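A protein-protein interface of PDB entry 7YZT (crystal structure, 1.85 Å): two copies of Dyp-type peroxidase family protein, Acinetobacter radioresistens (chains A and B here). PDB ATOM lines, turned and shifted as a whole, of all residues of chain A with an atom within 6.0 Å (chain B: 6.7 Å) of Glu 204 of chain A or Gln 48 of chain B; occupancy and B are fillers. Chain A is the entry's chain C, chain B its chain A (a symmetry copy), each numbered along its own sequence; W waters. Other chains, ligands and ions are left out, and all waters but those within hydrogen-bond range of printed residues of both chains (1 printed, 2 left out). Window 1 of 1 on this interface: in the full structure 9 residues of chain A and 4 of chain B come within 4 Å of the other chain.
Among the printed residues, merely in contact across the chains: Glu 204 of chain A with Arg 44 of chain B (3.0 Å), Ile 143 of chain A with Gln 48 of chain B (3.2 Å), Ser 205 of chain A with Arg 44 of chain B (3.3 Å), Asp 135 of chain A with Gln 48 of chain B (3.6 Å), Thr 146 of chain A with Thr 47 of chain B (3.7 Å), Ile 206 of chain A with Arg 44 of chain B (3.7 Å) and Glu 204 of chain A with Gln 48 of chain B (3.8 Å).
Hydrophobic or aromatic side chains of chain A within 4 Å of the printed part of chain B: Ile 143 and Ile 206.
Water W1 lies within hydrogen-bond range of OG1 of Thr 146 of chain A (2.8 Å) and O of Arg 44 of chain B (3.3 Å).
The backbone NH of Ser 205 of chain A lies within hydrogen-bond range of the side-chain hydroxyl of Thr 201 of chain A (3.2 Å). O of Asp 43 of chain B lies within hydrogen-bond range of OG1 of Thr 47 of chain B (3.2 Å). The side-chain carboxylate (OE1) of Glu 204 of chain A is in hydrogen-bond range of the side-chain hydroxyl (OG1) of Thr 201 of chain A (2.8 Å). O of Ile 206 of chain A sits at hydrogen-bond distance from N of Thr 201 of chain A. NE of Arg 137 of chain A is in salt-bridge range of OD1 of Asp 135 of chain A (2.9 Å). The side-chain hydroxyl of Thr 146 of chain A lies within hydrogen-bond range of the side-chain hydroxyl of Ser 205 of chain A (2.7 Å).
Glu 204 of chain A touches just these residues of chain B: Arg 44 and Gln 48. Gln 48 of chain B touches just these residues of chain A: Asp 135, Ile 143 and Glu 204. Of the printed residues of chain B, Ile 143 of chain A touches Gln 48. Printed residues of chain B within 4 Å of Ser 205 of chain A: Arg 44 (3.3 Å). Of the printed residues of chain B, Thr 146 of chain A touches Thr 47 (3.7 Å). Ala 51 of chain B touches none of the printed residues of chain A. Asp 43 of chain B touches none of the printed residues of chain A. The nearest residue of chain A that does not touch Gln 48 of chain B is Arg 132 of chain A (4.05 Å). The nearest printed residue of chain A that does not touch Thr 47 of chain B is Arg 132 of chain A (4.4 Å).
No position is printed for both chains.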
ATOM      1  N   ARG A 132      16.832  20.129  -4.434  1.00  0.00           N
ATOM      2  CA  ARG A 132      16.454  19.285  -3.306  1.00  0.00           C
ATOM      3  C   ARG A 132      15.089  19.712  -2.785  1.00  0.00           C
ATOM      4  O   ARG A 132      14.811  20.905  -2.625  1.00  0.00           O
ATOM      5  CB  ARG A 132      17.500  19.352  -2.191  1.00  0.00           C
ATOM      6  CG  ARG A 132      17.565  18.094  -1.292  1.00  0.00           C
ATOM      7  CD  ARG A 132      18.963  17.875  -0.660  1.00  0.00           C
ATOM      8  NE  ARG A 132      19.052  16.674   0.173  1.00  0.00           N
ATOM      9  CZ  ARG A 132      18.602  16.608   1.420  1.00  0.00           C
ATOM     10  NH1 ARG A 132      17.987  17.634   1.987  1.00  0.00           N
ATOM     11  NH2 ARG A 132      18.777  15.489   2.118  1.00  0.00           N
ATOM     12  N   ASP A 135      13.106  17.255   2.818  1.00  0.00           N
ATOM     13  CA  ASP A 135      14.164  16.431   3.409  1.00  0.00           C
ATOM     14  C   ASP A 135      14.551  15.294   2.457  1.00  0.00           C
ATOM     15  O   ASP A 135      14.352  14.114   2.731  1.00  0.00           O
ATOM     16  CB  ASP A 135      13.749  15.921   4.793  1.00  0.00           C
ATOM     17  CG  ASP A 135      12.314  15.357   4.840  1.00  0.00           C
ATOM     18  OD1 ASP A 135      11.389  15.961   4.251  1.00  0.00           O
ATOM     19  OD2 ASP A 135      12.097  14.345   5.544  1.00  0.00           O
ATOM     20  N   ARG A 137      13.254  14.444  -0.505  1.00  0.00           N
ATOM     21  CA  ARG A 137      12.110  13.680  -0.983  1.00  0.00           C
ATOM     22  C   ARG A 137      11.894  13.875  -2.479  1.00  0.00           C
ATOM     23  O   ARG A 137      12.296  14.885  -3.064  1.00  0.00           O
ATOM     24  CB  ARG A 137      10.832  14.074  -0.225  1.00  0.00           C
ATOM     25  CG  ARG A 137      10.858  13.656   1.240  1.00  0.00           C
ATOM     26  CD  ARG A 137       9.575  13.976   1.991  1.00  0.00           C
ATOM     27  NE  ARG A 137       9.789  13.743   3.411  1.00  0.00           N
ATOM     28  CZ  ARG A 137       9.540  12.590   4.016  1.00  0.00           C
ATOM     29  NH1 ARG A 137       8.953  11.591   3.376  1.00  0.00           N
ATOM     30  NH2 ARG A 137       9.898  12.434   5.285  1.00  0.00           N
ATOM     31  N   ILE A 143      10.934   9.664   0.482  1.00  0.00           N
ATOM     32  CA  ILE A 143      12.371   9.931   0.508  1.00  0.00           C
ATOM     33  C   ILE A 143      13.065   9.176  -0.619  1.00  0.00           C
ATOM     34  O   ILE A 143      12.850   7.971  -0.811  1.00  0.00           O
ATOM     35  CB  ILE A 143      12.953   9.552   1.877  1.00  0.00           C
ATOM     36  CG1 ILE A 143      12.449  10.524   2.958  1.00  0.00           C
ATOM     37  CG2 ILE A 143      14.487   9.569   1.855  1.00  0.00           C
ATOM     38  CD1 ILE A 143      12.587   9.988   4.367  1.00  0.00           C
ATOM     39  N   THR A 146      17.568   6.427   0.169  1.00  0.00           N
ATOM     40  CA  THR A 146      17.825   5.685   1.404  1.00  0.00           C
ATOM     41  C   THR A 146      18.870   4.583   1.214  1.00  0.00           C
ATOM     42  O   THR A 146      19.749   4.401   2.064  1.00  0.00           O
ATOM     43  CB  THR A 146      16.514   5.086   1.933  1.00  0.00           C
ATOM     44  OG1 THR A 146      15.563   6.132   2.157  1.00  0.00           O
ATOM     45  CG2 THR A 146      16.735   4.349   3.239  1.00  0.00           C
ATOM     46  N   GLU A 195       2.619   3.191  -0.042  1.00  0.00           N
ATOM     47  CA  GLU A 195       3.718   2.439   0.562  1.00  0.00           C
ATOM     48  C   GLU A 195       3.844   1.047  -0.067  1.00  0.00           C
ATOM     49  O   GLU A 195       4.961   0.548  -0.257  1.00  0.00           O
ATOM     50  CB  GLU A 195       3.528   2.370   2.084  1.00  0.00           C
ATOM     51  CG  GLU A 195       3.707   3.755   2.760  1.00  0.00           C
ATOM     52  CD  GLU A 195       3.439   3.780   4.277  1.00  0.00           C
ATOM     53  OE1 GLU A 195       2.820   2.846   4.820  1.00  0.00           O
ATOM     54  OE2 GLU A 195       3.841   4.767   4.929  1.00  0.00           O
ATOM     55  N   THR A 201       8.035   2.828   3.893  1.00  0.00           N
ATOM     56  CA  THR A 201       7.015   3.720   4.448  1.00  0.00           C
ATOM     57  C   THR A 201       7.245   5.151   3.955  1.00  0.00           C
ATOM     58  O   THR A 201       8.366   5.542   3.605  1.00  0.00           O
ATOM     59  CB  THR A 201       7.009   3.683   5.979  1.00  0.00           C
ATOM     60  OG1 THR A 201       8.227   4.254   6.479  1.00  0.00           O
ATOM     61  CG2 THR A 201       6.851   2.242   6.491  1.00  0.00           C
ATOM     62  N   LYS A 202       6.161   5.933   3.925  1.00  0.00           N
ATOM     63  CA  LYS A 202       6.223   7.280   3.360  1.00  0.00           C
ATOM     64  C   LYS A 202       6.964   8.253   4.279  1.00  0.00           C
ATOM     65  O   LYS A 202       7.890   8.946   3.839  1.00  0.00           O
ATOM     66  CB  LYS A 202       4.804   7.796   3.071  1.00  0.00           C
ATOM     67  CG  LYS A 202       4.777   9.076   2.249  1.00  0.00           C
ATOM     68  CD  LYS A 202       3.325   9.482   1.855  1.00  0.00           C
ATOM     69  CE  LYS A 202       3.364  10.576   0.770  1.00  0.00           C
ATOM     70  NZ  LYS A 202       2.006  10.925   0.249  1.00  0.00           N
ATOM     71  N   LEU A 203       6.543   8.364   5.540  1.00  0.00           N
ATOM     72  CA  LEU A 203       7.150   9.369   6.419  1.00  0.00           C
ATOM     73  C   LEU A 203       8.615   9.041   6.681  1.00  0.00           C
ATOM     74  O   LEU A 203       9.495   9.896   6.515  1.00  0.00           O
ATOM     75  CB  LEU A 203       6.389   9.478   7.742  1.00  0.00           C
ATOM     76  CG  LEU A 203       7.056  10.429   8.755  1.00  0.00           C
ATOM     77  CD1 LEU A 203       7.068  11.868   8.253  1.00  0.00           C
ATOM     78  CD2 LEU A 203       6.443  10.374  10.149  1.00  0.00           C
ATOM     79  N   GLU A 204       8.898   7.790   7.040  1.00  0.00           N
ATOM     80  CA  GLU A 204      10.206   7.415   7.560  1.00  0.00           C
ATOM     81  C   GLU A 204      11.114   6.740   6.544  1.00  0.00           C
ATOM     82  O   GLU A 204      12.330   6.731   6.753  1.00  0.00           O
ATOM     83  CB  GLU A 204      10.055   6.476   8.775  1.00  0.00           C
ATOM     84  CG  GLU A 204       9.081   6.955   9.857  1.00  0.00           C
ATOM     85  CD  GLU A 204       7.652   6.431   9.660  1.00  0.00           C
ATOM     86  OE1 GLU A 204       7.324   5.919   8.558  1.00  0.00           O
ATOM     87  OE2 GLU A 204       6.852   6.538  10.606  1.00  0.00           O
ATOM     88  N   SER A 205      10.573   6.182   5.457  1.00  0.00           N
ATOM     89  CA  SER A 205      11.357   5.358   4.530  1.00  0.00           C
ATOM     90  C   SER A 205      11.873   4.095   5.218  1.00  0.00           C
ATOM     91  O   SER A 205      12.979   3.628   4.948  1.00  0.00           O
ATOM     92  CB  SER A 205      12.515   6.150   3.911  1.00  0.00           C
ATOM     93  OG  SER A 205      12.954   5.583   2.694  1.00  0.00           O
ATOM     94  N   ILE A 206      11.072   3.532   6.116  1.00  0.00           N
ATOM     95  CA  ILE A 206      11.386   2.216   6.667  1.00  0.00           C
ATOM     96  C   ILE A 206      11.005   1.166   5.625  1.00  0.00           C
ATOM     97  O   ILE A 206       9.917   1.226   5.049  1.00  0.00           O
ATOM     98  CB  ILE A 206      10.652   1.990   8.000  1.00  0.00           C
ATOM     99  CG1 ILE A 206      11.205   2.923   9.086  1.00  0.00           C
ATOM    100  CG2 ILE A 206      10.767   0.545   8.438  1.00  0.00           C
ATOM    101  CD1 ILE A 206      10.359   2.977  10.352  1.00  0.00           C
ATOM    102  N   ASP B  43      21.452   4.197   9.920  1.00  0.00           N
ATOM    103  CA  ASP B  43      21.762   4.345   8.500  1.00  0.00           C
ATOM    104  C   ASP B  43      20.746   5.231   7.808  1.00  0.00           C
ATOM    105  O   ASP B  43      21.108   6.096   6.999  1.00  0.00           O
ATOM    106  CB  ASP B  43      21.796   2.974   7.821  1.00  0.00           C
ATOM    107  CG  ASP B  43      22.962   2.131   8.264  1.00  0.00           C
ATOM    108  OD1 ASP B  43      23.789   2.637   9.042  1.00  0.00           O
ATOM    109  OD2 ASP B  43      23.040   0.947   7.854  1.00  0.00           O
ATOM    110  N   ARG B  44      19.463   5.017   8.102  1.00  0.00           N
ATOM    111  CA  ARG B  44      18.399   5.775   7.461  1.00  0.00           C
ATOM    112  C   ARG B  44      18.471   7.253   7.825  1.00  0.00           C
ATOM    113  O   ARG B  44      18.267   8.125   6.969  1.00  0.00           O
ATOM    114  CB  ARG B  44      17.058   5.148   7.865  1.00  0.00           C
ATOM    115  CG  ARG B  44      15.853   5.704   7.187  1.00  0.00           C
ATOM    116  CD  ARG B  44      14.591   4.923   7.583  1.00  0.00           C
ATOM    117  NE  ARG B  44      14.616   4.305   8.905  1.00  0.00           N
ATOM    118  CZ  ARG B  44      14.176   4.866  10.024  1.00  0.00           C
ATOM    119  NH1 ARG B  44      13.703   6.103  10.044  1.00  0.00           N
ATOM    120  NH2 ARG B  44      14.202   4.165  11.152  1.00  0.00           N
ATOM    121  N   LEU B  45      18.784   7.559   9.089  1.00  0.00           N
ATOM    122  CA  LEU B  45      18.878   8.952   9.509  1.00  0.00           C
ATOM    123  C   LEU B  45      20.136   9.626   8.967  1.00  0.00           C
ATOM    124  O   LEU B  45      20.113  10.825   8.665  1.00  0.00           O
ATOM    125  CB  LEU B  45      18.819   9.025  11.038  1.00  0.00           C
ATOM    126  CG  LEU B  45      17.417   8.694  11.572  1.00  0.00           C
ATOM    127  CD1 LEU B  45      17.324   8.732  13.100  1.00  0.00           C
ATOM    128  CD2 LEU B  45      16.415   9.661  10.977  1.00  0.00           C
ATOM    129  N   ILE B  46      21.237   8.879   8.829  1.00  0.00           N
ATOM    130  CA  ILE B  46      22.440   9.461   8.245  1.00  0.00           C
ATOM    131  C   ILE B  46      22.155   9.969   6.840  1.00  0.00           C
ATOM    132  O   ILE B  46      22.601  11.060   6.460  1.00  0.00           O
ATOM    133  CB  ILE B  46      23.592   8.440   8.250  1.00  0.00           C
ATOM    134  CG1 ILE B  46      24.163   8.306   9.659  1.00  0.00           C
ATOM    135  CG2 ILE B  46      24.666   8.831   7.233  1.00  0.00           C
ATOM    136  CD1 ILE B  46      25.081   7.130   9.815  1.00  0.00           C
ATOM    137  N   THR B  47      21.402   9.189   6.051  1.00  0.00           N
ATOM    138  CA  THR B  47      21.083   9.587   4.681  1.00  0.00           C
ATOM    139  C   THR B  47      20.267  10.872   4.666  1.00  0.00           C
ATOM    140  O   THR B  47      20.442  11.722   3.784  1.00  0.00           O
ATOM    141  CB  THR B  47      20.303   8.479   3.960  1.00  0.00           C
ATOM    142  OG1 THR B  47      21.046   7.253   3.978  1.00  0.00           O
ATOM    143  CG2 THR B  47      20.030   8.881   2.498  1.00  0.00           C
ATOM    144  N   GLN B  48      19.364  11.025   5.630  1.00  0.00           N
ATOM    145  CA  GLN B  48      18.521  12.213   5.681  1.00  0.00           C
ATOM    146  C   GLN B  48      19.210  13.399   6.348  1.00  0.00           C
ATOM    147  O   GLN B  48      18.859  14.547   6.054  1.00  0.00           O
ATOM    148  CB  GLN B  48      17.220  11.901   6.420  1.00  0.00           C
ATOM    149  CG  GLN B  48      16.382  10.807   5.783  1.00  0.00           C
ATOM    150  CD  GLN B  48      15.089  10.606   6.538  1.00  0.00           C
ATOM    151  OE1 GLN B  48      14.856   9.546   7.138  1.00  0.00           O
ATOM    152  NE2 GLN B  48      14.247  11.650   6.556  1.00  0.00           N
ATOM    153  N   HIS B  49      20.176  13.157   7.241  1.00  0.00           N
ATOM    154  CA  HIS B  49      20.846  14.235   7.976  1.00  0.00           C
ATOM    155  C   HIS B  49      22.351  14.004   7.997  1.00  0.00           C
ATOM    156  O   HIS B  49      22.946  13.793   9.055  1.00  0.00           O
ATOM    157  CB  HIS B  49      20.298  14.331   9.399  1.00  0.00           C
ATOM    158  CG  HIS B  49      18.807  14.371   9.473  1.00  0.00           C
ATOM    159  ND1 HIS B  49      18.072  15.476   9.094  1.00  0.00           N
ATOM    160  CD2 HIS B  49      17.910  13.443   9.883  1.00  0.00           C
ATOM    161  CE1 HIS B  49      16.787  15.226   9.268  1.00  0.00           C
ATOM    162  NE2 HIS B  49      16.662  14.001   9.752  1.00  0.00           N
ATOM    163  N   PRO B  50      23.013  14.052   6.841  1.00  0.00           N
ATOM    164  CA  PRO B  50      24.446  13.721   6.812  1.00  0.00           C
ATOM    165  C   PRO B  50      25.317  14.685   7.606  1.00  0.00           C
ATOM    166  O   PRO B  50      26.476  14.355   7.890  1.00  0.00           O
ATOM    167  CB  PRO B  50      24.780  13.752   5.314  1.00  0.00           C
ATOM    168  CG  PRO B  50      23.793  14.723   4.756  1.00  0.00           C
ATOM    169  CD  PRO B  50      22.518  14.431   5.508  1.00  0.00           C
ATOM    170  N   ALA B  51      24.802  15.846   7.997  1.00  0.00           N
ATOM    171  CA  ALA B  51      25.556  16.789   8.813  1.00  0.00           C
ATOM    172  C   ALA B  51      25.248  16.697  10.309  1.00  0.00           C
ATOM    173  O   ALA B  51      25.810  17.472  11.088  1.00  0.00           O
ATOM    174  CB  ALA B  51      25.294  18.215   8.325  1.00  0.00           C
ATOM    175  N   ILE B  54      25.722  11.680  13.244  1.00  0.00           N
ATOM    176  CA  ILE B  54      25.031  10.533  13.824  1.00  0.00           C
ATOM    177  C   ILE B  54      26.022   9.387  13.975  1.00  0.00           C
ATOM    178  O   ILE B  54      26.545   8.866  12.979  1.00  0.00           O
ATOM    179  CB  ILE B  54      23.831  10.125  12.959  1.00  0.00           C
ATOM    180  CG1 ILE B  54      22.930  11.338  12.717  1.00  0.00           C
ATOM    181  CG2 ILE B  54      23.076   8.968  13.602  1.00  0.00           C
ATOM    182  CD1 ILE B  54      21.692  11.014  11.916  1.00  0.00           C
HETATM  183  O   HOH W   1      16.677   7.906   4.073  1.00  0.00           O
